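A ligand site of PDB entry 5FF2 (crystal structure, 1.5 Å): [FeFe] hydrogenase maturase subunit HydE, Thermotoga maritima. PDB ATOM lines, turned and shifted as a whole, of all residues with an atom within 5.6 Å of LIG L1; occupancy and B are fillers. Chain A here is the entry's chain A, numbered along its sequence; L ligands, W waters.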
ATOM      1  N   CYS A  63       6.385  25.479   8.833  1.00  0.00           N
ATOM      2  CA  CYS A  63       5.959  24.306   8.124  1.00  0.00           C
ATOM      3  C   CYS A  63       4.463  24.012   8.352  1.00  0.00           C
ATOM      4  O   CYS A  63       3.953  24.090   9.466  1.00  0.00           O
ATOM      5  CB  CYS A  63       6.775  23.059   8.501  1.00  0.00           C
ATOM      6  SG  CYS A  63       6.574  21.691   7.347  1.00  0.00           S
ATOM      7  N   TYR A  69       8.735  13.106  13.740  1.00  0.00           N
ATOM      8  CA  TYR A  69      10.167  13.192  14.125  1.00  0.00           C
ATOM      9  C   TYR A  69      10.739  14.590  14.161  1.00  0.00           C
ATOM     10  O   TYR A  69      11.774  14.799  14.791  1.00  0.00           O
ATOM     11  CB  TYR A  69      11.029  12.309  13.195  1.00  0.00           C
ATOM     12  CG  TYR A  69      10.732  12.477  11.746  1.00  0.00           C
ATOM     13  CD1 TYR A  69      11.248  13.557  11.029  1.00  0.00           C
ATOM     14  CD2 TYR A  69       9.908  11.572  11.010  1.00  0.00           C
ATOM     15  CE1 TYR A  69      10.925  13.731   9.687  1.00  0.00           C
ATOM     16  CE2 TYR A  69       9.638  11.747   9.678  1.00  0.00           C
ATOM     17  CZ  TYR A  69      10.139  12.811   8.991  1.00  0.00           C
ATOM     18  OH  TYR A  69       9.817  12.949   7.700  1.00  0.00           O
ATOM     19  N   CYS A  70      10.063  15.573  13.526  1.00  0.00           N
ATOM     20  CA  CYS A  70      10.688  16.801  13.203  1.00  0.00           C
ATOM     21  C   CYS A  70      10.360  17.955  14.135  1.00  0.00           C
ATOM     22  O   CYS A  70       9.157  18.229  14.372  1.00  0.00           O
ATOM     23  CB  CYS A  70      10.275  17.223  11.808  1.00  0.00           C
ATOM     24  SG  CYS A  70      11.085  18.719  11.164  1.00  0.00           S
ATOM     25  N   GLY A  71      11.354  18.675  14.616  1.00  0.00           N
ATOM     26  CA  GLY A  71      11.135  19.812  15.472  1.00  0.00           C
ATOM     27  C   GLY A  71      10.388  20.985  14.863  1.00  0.00           C
ATOM     28  O   GLY A  71       9.840  21.832  15.575  1.00  0.00           O
ATOM     29  N   GLN A 107      16.871  25.579   1.704  1.00  0.00           N
ATOM     30  CA  GLN A 107      16.058  24.628   2.462  1.00  0.00           C
ATOM     31  C   GLN A 107      15.102  25.339   3.374  1.00  0.00           C
ATOM     32  O   GLN A 107      15.442  26.365   3.970  1.00  0.00           O
ATOM     33  CB  GLN A 107      16.929  23.649   3.225  1.00  0.00           C
ATOM     34  CG  GLN A 107      16.095  22.468   3.802  1.00  0.00           C
ATOM     35  CD  GLN A 107      16.956  21.464   4.493  1.00  0.00           C
ATOM     36  OE1 GLN A 107      17.299  21.676   5.666  1.00  0.00           O
ATOM     37  NE2 GLN A 107      17.312  20.392   3.843  1.00  0.00           N
ATOM     38  N   SER A 108      13.904  24.766   3.531  1.00  0.00           N
ATOM     39  CA  SER A 108      12.911  25.315   4.440  1.00  0.00           C
ATOM     40  C   SER A 108      11.953  24.225   4.890  1.00  0.00           C
ATOM     41  O   SER A 108      11.880  23.152   4.274  1.00  0.00           O
ATOM     42  CB  SER A 108      12.101  26.450   3.778  1.00  0.00           C
ATOM     43  OG  SER A 108      11.429  25.992   2.644  1.00  0.00           O
ATOM     44  N   GLY A 109      11.171  24.574   5.919  1.00  0.00           N
ATOM     45  CA  GLY A 109       9.947  23.858   6.152  1.00  0.00           C
ATOM     46  C   GLY A 109       9.047  24.070   4.922  1.00  0.00           C
ATOM     47  O   GLY A 109       9.320  24.910   4.032  1.00  0.00           O
ATOM     48  N   GLU A 110       7.961  23.310   4.851  1.00  0.00           N
ATOM     49  CA  GLU A 110       6.973  23.518   3.799  1.00  0.00           C
ATOM     50  C   GLU A 110       6.150  24.761   4.119  1.00  0.00           C
ATOM     51  O   GLU A 110       5.057  24.712   4.718  1.00  0.00           O
ATOM     52  CB  GLU A 110       6.063  22.295   3.592  1.00  0.00           C
ATOM     53  CG  GLU A 110       6.785  21.105   3.008  1.00  0.00           C
ATOM     54  CD  GLU A 110       5.853  20.037   2.503  1.00  0.00           C
ATOM     55  OE1 GLU A 110       4.630  20.245   2.466  1.00  0.00           O
ATOM     56  OE2 GLU A 110       6.329  18.944   2.107  1.00  0.00           O
ATOM     57  N   SER A 136      15.458  22.411  -1.518  1.00  0.00           N
ATOM     58  CA  SER A 136      15.006  21.350  -0.591  1.00  0.00           C
ATOM     59  C   SER A 136      13.816  21.918   0.167  1.00  0.00           C
ATOM     60  O   SER A 136      13.923  22.348   1.297  1.00  0.00           O
ATOM     61  CB  SER A 136      16.149  20.947   0.300  1.00  0.00           C
ATOM     62  OG  SER A 136      15.820  19.894   1.185  1.00  0.00           O
ATOM     63  N   LEU A 137      12.652  21.942  -0.514  1.00  0.00           N
ATOM     64  CA  LEU A 137      11.433  22.633  -0.021  1.00  0.00           C
ATOM     65  C   LEU A 137      10.274  21.716   0.301  1.00  0.00           C
ATOM     66  O   LEU A 137       9.223  22.188   0.676  1.00  0.00           O
ATOM     67  CB  LEU A 137      11.012  23.688  -1.044  1.00  0.00           C
ATOM     68  CG  LEU A 137      12.119  24.634  -1.563  1.00  0.00           C
ATOM     69  CD1 LEU A 137      11.558  25.580  -2.600  1.00  0.00           C
ATOM     70  CD2 LEU A 137      12.811  25.359  -0.441  1.00  0.00           C
ATOM     71  N   GLY A 138      10.500  20.394   0.137  1.00  0.00           N
ATOM     72  CA  GLY A 138       9.381  19.448   0.419  1.00  0.00           C
ATOM     73  C   GLY A 138       8.568  19.111  -0.806  1.00  0.00           C
ATOM     74  O   GLY A 138       9.025  19.229  -1.956  1.00  0.00           O
ATOM     75  N   LEU A 157      16.585  18.161  -3.449  1.00  0.00           N
ATOM     76  CA  LEU A 157      16.723  17.154  -2.414  1.00  0.00           C
ATOM     77  C   LEU A 157      15.392  16.836  -1.790  1.00  0.00           C
ATOM     78  O   LEU A 157      14.723  17.755  -1.277  1.00  0.00           O
ATOM     79  CB  LEU A 157      17.695  17.658  -1.300  1.00  0.00           C
ATOM     80  CG  LEU A 157      19.051  18.212  -1.764  1.00  0.00           C
ATOM     81  CD1 LEU A 157      19.788  18.747  -0.579  1.00  0.00           C
ATOM     82  CD2 LEU A 157      19.828  17.172  -2.537  1.00  0.00           C
ATOM     83  N   LEU A 158      15.021  15.588  -1.839  1.00  0.00           N
ATOM     84  CA  LEU A 158      13.735  15.127  -1.230  1.00  0.00           C
ATOM     85  C   LEU A 158      13.963  13.754  -0.693  1.00  0.00           C
ATOM     86  O   LEU A 158      13.712  12.749  -1.338  1.00  0.00           O
ATOM     87  CB  LEU A 158      12.584  15.258  -2.199  1.00  0.00           C
ATOM     88  CG  LEU A 158      11.192  15.076  -1.632  1.00  0.00           C
ATOM     89  CD1 LEU A 158      10.822  16.319  -0.875  1.00  0.00           C
ATOM     90  CD2 LEU A 158      10.214  14.767  -2.758  1.00  0.00           C
ATOM     91  N   ARG A 159      14.431  13.663   0.526  1.00  0.00           N
ATOM     92  CA  ARG A 159      14.748  12.363   1.118  1.00  0.00           C
ATOM     93  C   ARG A 159      13.466  11.531   1.130  1.00  0.00           C
ATOM     94  O   ARG A 159      12.403  12.021   1.422  1.00  0.00           O
ATOM     95  CB  ARG A 159      15.213  12.468   2.541  1.00  0.00           C
ATOM     96  CG  ARG A 159      16.665  12.977   2.587  1.00  0.00           C
ATOM     97  CD  ARG A 159      16.995  13.027   4.086  1.00  0.00           C
ATOM     98  NE  ARG A 159      18.333  13.480   4.298  1.00  0.00           N
ATOM     99  CZ  ARG A 159      18.962  13.292   5.438  1.00  0.00           C
ATOM    100  NH1 ARG A 159      18.322  12.699   6.448  1.00  0.00           N
ATOM    101  NH2 ARG A 159      20.213  13.720   5.540  1.00  0.00           N
ATOM    102  N   GLU A 161      12.942   9.187   3.176  1.00  0.00           N
ATOM    103  CA  GLU A 161      12.747   9.062   4.644  1.00  0.00           C
ATOM    104  C   GLU A 161      12.754   7.585   5.120  1.00  0.00           C
ATOM    105  O   GLU A 161      13.580   7.234   5.950  1.00  0.00           O
ATOM    106  CB  GLU A 161      11.499   9.809   5.131  1.00  0.00           C
ATOM    107  CG  GLU A 161      11.363  11.217   4.589  1.00  0.00           C
ATOM    108  CD  GLU A 161      12.516  12.175   5.050  1.00  0.00           C
ATOM    109  OE1 GLU A 161      13.511  11.734   5.719  1.00  0.00           O
ATOM    110  OE2 GLU A 161      12.352  13.370   4.748  1.00  0.00           O
ATOM    111  N   ARG A 172       4.565  10.366   8.891  1.00  0.00           N
ATOM    112  CA  ARG A 172       4.291  11.539   8.054  1.00  0.00           C
ATOM    113  C   ARG A 172       2.797  11.578   7.690  1.00  0.00           C
ATOM    114  O   ARG A 172       2.415  11.273   6.556  1.00  0.00           O
ATOM    115  CB  ARG A 172       5.213  11.497   6.847  1.00  0.00           C
ATOM    116  CG  ARG A 172       6.672  11.316   7.243  1.00  0.00           C
ATOM    117  CD  ARG A 172       7.630  11.424   6.069  1.00  0.00           C
ATOM    118  NE  ARG A 172       7.656  12.841   5.631  1.00  0.00           N
ATOM    119  CZ  ARG A 172       7.186  13.330   4.497  1.00  0.00           C
ATOM    120  NH1 ARG A 172       6.812  12.589   3.553  1.00  0.00           N
ATOM    121  NH2 ARG A 172       7.128  14.651   4.385  1.00  0.00           N
ATOM    122  N   ARG A 180       5.513  10.793  -1.947  1.00  0.00           N
ATOM    123  CA  ARG A 180       6.941  11.145  -1.906  1.00  0.00           C
ATOM    124  C   ARG A 180       7.677  10.630  -3.142  1.00  0.00           C
ATOM    125  O   ARG A 180       8.449  11.347  -3.765  1.00  0.00           O
ATOM    126  CB  ARG A 180       7.564  10.570  -0.637  1.00  0.00           C
ATOM    127  CG  ARG A 180       8.923  11.172  -0.232  1.00  0.00           C
ATOM    128  CD  ARG A 180       8.701  12.475   0.448  1.00  0.00           C
ATOM    129  NE  ARG A 180       9.893  12.991   1.075  1.00  0.00           N
ATOM    130  CZ  ARG A 180       9.959  14.214   1.639  1.00  0.00           C
ATOM    131  NH1 ARG A 180       8.900  15.018   1.663  1.00  0.00           N
ATOM    132  NH2 ARG A 180      11.126  14.625   2.173  1.00  0.00           N
ATOM    133  N   SER A 198      17.440   8.687   3.540  1.00  0.00           N
ATOM    134  CA  SER A 198      16.547   8.192   4.608  1.00  0.00           C
ATOM    135  C   SER A 198      17.218   8.440   5.939  1.00  0.00           C
ATOM    136  O   SER A 198      18.425   8.740   6.023  1.00  0.00           O
ATOM    137  CB  SER A 198      16.283   6.720   4.418  1.00  0.00           C
ATOM    138  OG  SER A 198      17.521   6.004   4.240  1.00  0.00           O
ATOM    139  N   MET A 199      16.414   8.324   6.982  1.00  0.00           N
ATOM    140  CA  MET A 199      16.906   8.289   8.349  1.00  0.00           C
ATOM    141  C   MET A 199      17.089   6.840   8.780  1.00  0.00           C
ATOM    142  O   MET A 199      16.416   5.933   8.301  1.00  0.00           O
ATOM    143  CB  MET A 199      15.980   8.988   9.305  1.00  0.00           C
ATOM    144  CG  MET A 199      15.967  10.540   9.117  1.00  0.00           C
ATOM    145  SD  MET A 199      14.722  11.356  10.173  1.00  0.00           S
ATOM    146  CE  MET A 199      13.257  11.034   9.187  1.00  0.00           C
ATOM    147  N   PRO A 229      21.333   9.689  10.984  1.00  0.00           N
ATOM    148  CA  PRO A 229      20.564   9.024  12.047  1.00  0.00           C
ATOM    149  C   PRO A 229      19.313   9.858  12.395  1.00  0.00           C
ATOM    150  O   PRO A 229      19.322  11.027  12.317  1.00  0.00           O
ATOM    151  CB  PRO A 229      21.582   8.991  13.220  1.00  0.00           C
ATOM    152  CG  PRO A 229      22.304  10.285  13.067  1.00  0.00           C
ATOM    153  CD  PRO A 229      22.542  10.370  11.550  1.00  0.00           C
ATOM    154  N   PHE A 230      18.272   9.169  12.834  1.00  0.00           N
ATOM    155  CA  PHE A 230      17.190   9.808  13.569  1.00  0.00           C
ATOM    156  C   PHE A 230      17.719  10.312  14.902  1.00  0.00           C
ATOM    157  O   PHE A 230      18.344   9.604  15.682  1.00  0.00           O
ATOM    158  CB  PHE A 230      16.058   8.794  13.826  1.00  0.00           C
ATOM    159  CG  PHE A 230      15.058   9.239  14.866  1.00  0.00           C
ATOM    160  CD1 PHE A 230      14.231  10.358  14.655  1.00  0.00           C
ATOM    161  CD2 PHE A 230      14.946   8.557  16.083  1.00  0.00           C
ATOM    162  CE1 PHE A 230      13.369  10.793  15.650  1.00  0.00           C
ATOM    163  CE2 PHE A 230      14.044   8.995  17.067  1.00  0.00           C
ATOM    164  CZ  PHE A 230      13.266  10.082  16.835  1.00  0.00           C
ATOM    165  N   ILE A 231      17.434  11.584  15.173  1.00  0.00           N
ATOM    166  CA  ILE A 231      17.755  12.210  16.446  1.00  0.00           C
ATOM    167  C   ILE A 231      16.487  12.752  17.115  1.00  0.00           C
ATOM    168  O   ILE A 231      15.824  13.657  16.585  1.00  0.00           O
ATOM    169  CB  ILE A 231      18.794  13.346  16.290  1.00  0.00           C
ATOM    170  CG1 ILE A 231      20.104  12.807  15.587  1.00  0.00           C
ATOM    171  CG2 ILE A 231      19.132  14.074  17.619  1.00  0.00           C
ATOM    172  CD1 ILE A 231      21.058  13.865  15.130  1.00  0.00           C
ATOM    173  N   PRO A 232      16.105  12.157  18.267  1.00  0.00           N
ATOM    174  CA  PRO A 232      14.829  12.569  18.848  1.00  0.00           C
ATOM    175  C   PRO A 232      14.827  14.041  19.305  1.00  0.00           C
ATOM    176  O   PRO A 232      15.825  14.554  19.828  1.00  0.00           O
ATOM    177  CB  PRO A 232      14.703  11.602  20.029  1.00  0.00           C
ATOM    178  CG  PRO A 232      16.145  11.321  20.418  1.00  0.00           C
ATOM    179  CD  PRO A 232      16.869  11.251  19.117  1.00  0.00           C
ATOM    180  N   HIS A 233      13.707  14.716  19.112  1.00  0.00           N
ATOM    181  CA  HIS A 233      13.537  16.096  19.464  1.00  0.00           C
ATOM    182  C   HIS A 233      12.511  16.182  20.595  1.00  0.00           C
ATOM    183  O   HIS A 233      11.431  15.603  20.523  1.00  0.00           O
ATOM    184  CB  HIS A 233      13.049  16.885  18.263  1.00  0.00           C
ATOM    185  CG  HIS A 233      13.036  18.368  18.454  1.00  0.00           C
ATOM    186  ND1 HIS A 233      12.245  19.025  19.383  1.00  0.00           N
ATOM    187  CD2 HIS A 233      13.740  19.345  17.837  1.00  0.00           C
ATOM    188  CE1 HIS A 233      12.430  20.328  19.301  1.00  0.00           C
ATOM    189  NE2 HIS A 233      13.347  20.542  18.393  1.00  0.00           N
ATOM    190  N   ALA A 270      23.714  15.700  10.777  1.00  0.00           N
ATOM    191  CA  ALA A 270      23.221  14.798  11.788  1.00  0.00           C
ATOM    192  C   ALA A 270      24.331  13.800  12.220  1.00  0.00           C
ATOM    193  O   ALA A 270      24.463  13.450  13.401  1.00  0.00           O
ATOM    194  CB  ALA A 270      21.955  14.100  11.335  1.00  0.00           C
ATOM    195  N   TYR A 303      16.356  26.869  13.554  1.00  0.00           N
ATOM    196  CA  TYR A 303      16.142  25.799  12.584  1.00  0.00           C
ATOM    197  C   TYR A 303      16.594  24.518  13.150  1.00  0.00           C
ATOM    198  O   TYR A 303      17.685  24.066  12.933  1.00  0.00           O
ATOM    199  CB  TYR A 303      16.781  26.134  11.263  1.00  0.00           C
ATOM    200  CG  TYR A 303      16.277  25.287  10.112  1.00  0.00           C
ATOM    201  CD1 TYR A 303      15.175  25.661   9.372  1.00  0.00           C
ATOM    202  CD2 TYR A 303      16.918  24.105   9.784  1.00  0.00           C
ATOM    203  CE1 TYR A 303      14.734  24.915   8.276  1.00  0.00           C
ATOM    204  CE2 TYR A 303      16.527  23.354   8.719  1.00  0.00           C
ATOM    205  CZ  TYR A 303      15.404  23.745   7.996  1.00  0.00           C
ATOM    206  OH  TYR A 303      14.976  23.020   6.862  1.00  0.00           O
ATOM    207  N   LEU A 305      15.530  20.872  13.360  1.00  0.00           N
ATOM    208  CA  LEU A 305      14.892  19.641  12.951  1.00  0.00           C
ATOM    209  C   LEU A 305      15.087  18.677  14.092  1.00  0.00           C
ATOM    210  O   LEU A 305      14.190  17.971  14.433  1.00  0.00           O
ATOM    211  CB  LEU A 305      15.588  19.146  11.666  1.00  0.00           C
ATOM    212  CG  LEU A 305      15.591  20.078  10.475  1.00  0.00           C
ATOM    213  CD1 LEU A 305      16.479  19.422   9.386  1.00  0.00           C
ATOM    214  CD2 LEU A 305      14.200  20.289   9.981  1.00  0.00           C
ATOM    215  N   TYR A 306      16.273  18.657  14.650  1.00  0.00           N
ATOM    216  CA  TYR A 306      16.679  17.896  15.783  1.00  0.00           C
ATOM    217  C   TYR A 306      17.527  18.778  16.679  1.00  0.00           C
ATOM    218  O   TYR A 306      18.086  19.814  16.175  1.00  0.00           O
ATOM    219  CB  TYR A 306      17.428  16.642  15.393  1.00  0.00           C
ATOM    220  CG  TYR A 306      18.591  16.879  14.443  1.00  0.00           C
ATOM    221  CD1 TYR A 306      19.826  17.221  14.930  1.00  0.00           C
ATOM    222  CD2 TYR A 306      18.416  16.781  13.100  1.00  0.00           C
ATOM    223  CE1 TYR A 306      20.867  17.459  14.110  1.00  0.00           C
ATOM    224  CE2 TYR A 306      19.452  17.022  12.224  1.00  0.00           C
ATOM    225  CZ  TYR A 306      20.695  17.349  12.735  1.00  0.00           C
ATOM    226  OH  TYR A 306      21.713  17.647  11.922  1.00  0.00           O
HETATM  227  N1  LIG L   1      10.722  20.128   4.574  1.00  0.00           N
HETATM  228  C1  LIG L   1      11.681  19.512   3.694  1.00  0.00           C
HETATM  229  C2  LIG L   1      13.068  19.877   4.068  1.00  0.00           C
HETATM  230  C3  LIG L   1      13.510  20.183   5.487  1.00  0.00           C
HETATM  231  S1  LIG L   1      13.649  18.679   6.413  1.00  0.00           S
HETATM  232  C4  LIG L   1      11.462  18.062   3.649  1.00  0.00           C
HETATM  233  O1  LIG L   1      11.996  17.516   2.666  1.00  0.00           O
HETATM  234  O2  LIG L   1      10.816  17.470   4.553  1.00  0.00           O
HETATM  235  C5  LIG L   1      15.217  17.985   5.917  1.00  0.00           C
HETATM  236  C6  LIG L   1      15.428  16.566   6.383  1.00  0.00           C
HETATM  237  O3  LIG L   1      15.799  16.536   7.787  1.00  0.00           O
HETATM  238  C7  LIG L   1      14.320  15.527   6.329  1.00  0.00           C
HETATM  239  O4  LIG L   1      14.270  14.977   5.002  1.00  0.00           O
HETATM  240  C8  LIG L   1      14.704  14.515   7.413  1.00  0.00           C
HETATM  241  O5  LIG L   1      15.264  13.284   6.910  1.00  0.00           O
HETATM  242  C9  LIG L   1      15.653  15.276   8.340  1.00  0.00           C
HETATM  243  N2  LIG L   1      15.170  15.334   9.686  1.00  0.00           N
HETATM  244  C10 LIG L   1      14.006  15.915  10.158  1.00  0.00           C
HETATM  245  N3  LIG L   1      13.837  15.659  11.467  1.00  0.00           N
HETATM  246  C11 LIG L   1      14.868  14.882  11.839  1.00  0.00           C
HETATM  247  C12 LIG L   1      15.301  14.327  13.089  1.00  0.00           C
HETATM  248  N4  LIG L   1      14.578  14.429  14.205  1.00  0.00           N
HETATM  249  N5  LIG L   1      16.438  13.622  13.103  1.00  0.00           N
HETATM  250  C13 LIG L   1      17.209  13.532  11.981  1.00  0.00           C
HETATM  251  N6  LIG L   1      16.862  14.037  10.845  1.00  0.00           N
HETATM  252  C14 LIG L   1      15.746  14.727  10.696  1.00  0.00           C
HETATM  253 FE1  LG2 L   2       9.965  18.829   9.165  1.00  0.00          FE
HETATM  254 FE2  LG2 L   2       8.033  20.028   7.762  1.00  0.00          FE
HETATM  255 FE3  LG2 L   2       8.203  17.285   7.860  1.00  0.00          FE
HETATM  256 FE4  LG2 L   2      10.188  18.780   6.371  1.00  0.00          FE
HETATM  257  S1  LG2 L   2       7.839  18.574   5.978  1.00  0.00           S
HETATM  258  S2  LG2 L   2      10.437  17.002   7.883  1.00  0.00           S
HETATM  259  S3  LG2 L   2      10.254  20.596   7.893  1.00  0.00           S
HETATM  260  S4  LG2 L   2       7.697  18.699   9.588  1.00  0.00           S
HETATM  261  C1  LG3 L   3      20.802  17.393   4.662  1.00  0.00           C
HETATM  262  C2  LG3 L   3      20.790  17.714   7.093  1.00  0.00           C
HETATM  263  C3  LG3 L   3      19.280  17.465   6.955  1.00  0.00           C
HETATM  264  S1  LG3 L   3      19.063  17.435   5.148  1.00  0.00           S
HETATM  265  O1  LG3 L   3      21.041  18.065   9.419  1.00  0.00           O
HETATM  266  C4  LG3 L   3      21.268  17.299   8.498  1.00  0.00           C
HETATM  267  O2  LG3 L   3      21.869  16.265   8.618  1.00  0.00           O
HETATM  268  C5  LG3 L   3      21.052  16.394   3.509  1.00  0.00           C
HETATM  269  O3  LG3 L   3      20.876  16.765   2.365  1.00  0.00           O
HETATM  270  O4  LG3 L   3      21.419  15.293   3.751  1.00  0.00           O
HETATM  271  N1  LG3 L   3      21.397  17.055   5.961  1.00  0.00           N
HETATM  272  O   HOH W   1       8.292  17.326   2.961  1.00  0.00           O
HETATM  273  O   HOH W   2      14.321  15.938   2.446  1.00  0.00           O
HETATM  274  O   HOH W   3      10.137  14.727   5.633  1.00  0.00           O
HETATM  275  O   HOH W   4      19.048  12.644   9.574  1.00  0.00           O
HETATM  276  O   HOH W   5      13.150  18.949   0.591  1.00  0.00           O
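The guanidinium group (NE) of Arg 180 sits at hydrogen-bond distance from the backbone carbonyl oxygen (O) of Arg 159. The side-chain hydroxyl of Tyr 306 sits at hydrogen-bond distance from the backbone NH of Ala 270 (3.0 Å). OH of Tyr 303 lies within hydrogen-bond range of OE1 of Gln 107. The backbone carbonyl oxygen (O) of Leu 305 is in hydrogen-bond range of the backbone NH (N) of Gly 71, at 2.9 Å. The guanidinium group of Arg 172 is in hydrogen-bond range of the side-chain hydroxyl of Tyr 69, at 3.0 Å. The backbone carbonyl oxygen (O) of Glu 161 is in hydrogen-bond range of the backbone NH (N) of Met 199. The side-chain hydroxyl (OG) of Ser 136 sits at hydrogen-bond distance from the side-chain amide nitrogen (NE2) of Gln 107 (3.1 Å). OE2 of Glu 161 lies within salt-bridge range of NH2 of Arg 180.
Water W2 lies within hydrogen-bond range of an oxygen (O4) of LIG L1 (2.7 Å), the backbone NH of Arg 159 (3.0 Å) and the guanidinium group of Arg 180 (3.5 Å). Water W5 lies within hydrogen-bond range of O of Leu 157, O1 of LIG L1, OG of Ser 136, N of Gly 138 and N of Leu 137. Water W4 lies within hydrogen-bond range of a nitrogen (N6) of LIG L1 (2.9 Å), the backbone carbonyl oxygen (O) of Pro 229 (3.2 Å) and the guanidinium group (NH1) of Arg 159 (3.2 Å). Water W1 lies within hydrogen-bond range of the side-chain carboxylate (OE2) of Glu 110 (2.7 Å), the guanidinium group (NH1) of Arg 180 (2.7 Å), the guanidinium group (NH2) of Arg 172 (3.2 Å) and a sulfur (S1) of LG2 L2 (3.3 Å). Water W3 lies within hydrogen-bond range of the side-chain carboxylate of Glu 161, the side-chain hydroxyl of Tyr 69, the guanidinium group of Arg 172 and a sulfur (S2) of LG2 L2.
The side-chain carboxylate (OE2) of Glu 161 is in hydrogen-bond range of an oxygen (O4) of LIG L1, 2.5 Å away. The side-chain sulfur (SG) of Cys 70 binds an iron atom (FE1) of LG2 L2, at 2.3 Å. The backbone carbonyl oxygen (O) of Ser 108 sits close to a nitrogen (N1) of LIG L1 (3.3 Å). The side-chain sulfur (SG) of Cys 63 is bound to an iron atom (FE2) of LG2 L2, at 2.3 Å. The guanidinium group (NH2) of Arg 159 lies within salt-bridge range of an oxygen (O4) of LG3 L3, at 2.7 Å. The guanidinium group (NH1) of Arg 159 is in hydrogen-bond range of an oxygen (O5) of LIG L1, 3.1 Å away. The side-chain hydroxyl (OH) of Tyr 306 is in hydrogen-bond range of an oxygen (O1) of LG3 L3. The backbone carbonyl oxygen of Tyr 69 sits at hydrogen-bond distance from a nitrogen (N4) of LIG L1, 2.9 Å away. The guanidinium group (NH2) of Arg 180 lies within salt-bridge range of an oxygen (O1) of LIG L1 (3.1 Å). The backbone NH of Ala 270 is in hydrogen-bond range of an oxygen (O2) of LG3 L3 (2.9 Å). The backbone NH (N) of Ile 231 lies within hydrogen-bond range of a nitrogen (N5) of LIG L1 (3.1 Å). A sulfur (S1) of LG3 L3 sits close to the side-chain amide nitrogen (NE2) of Gln 107 (3.7 Å). The backbone carbonyl oxygen (O) of Ile 231 lies within hydrogen-bond range of a nitrogen (N4) of LIG L1 (2.8 Å).
A nitrogen (N1) of LIG L1 is bound to an iron atom (FE4) of LG2 L2 (2.3 Å).
The side-chain sulfur of Met 199 lies close to a nitrogen (N6) of LIG L1. Merely in contact with LIG L1: Pro 229 (3.3 Å), Leu 305 (3.4 Å), Tyr 303 (3.5 Å), Tyr 306 (3.6 Å), Cys 70 (3.8 Å), Gln 107 (3.8 Å), Ser 136 (3.8 Å), Gly 138 (3.9 Å), Phe 230 (3.9 Å) and Leu 158 (3.9 Å). Hydrophobic or aromatic side chains within 4 Å of LIG L1: Tyr 69, Leu 158, Met 199, Ile 231, Leu 305 and Tyr 306. The nearest printed residue that does not touch LIG L1 is Gly 109 (4.1 Å).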
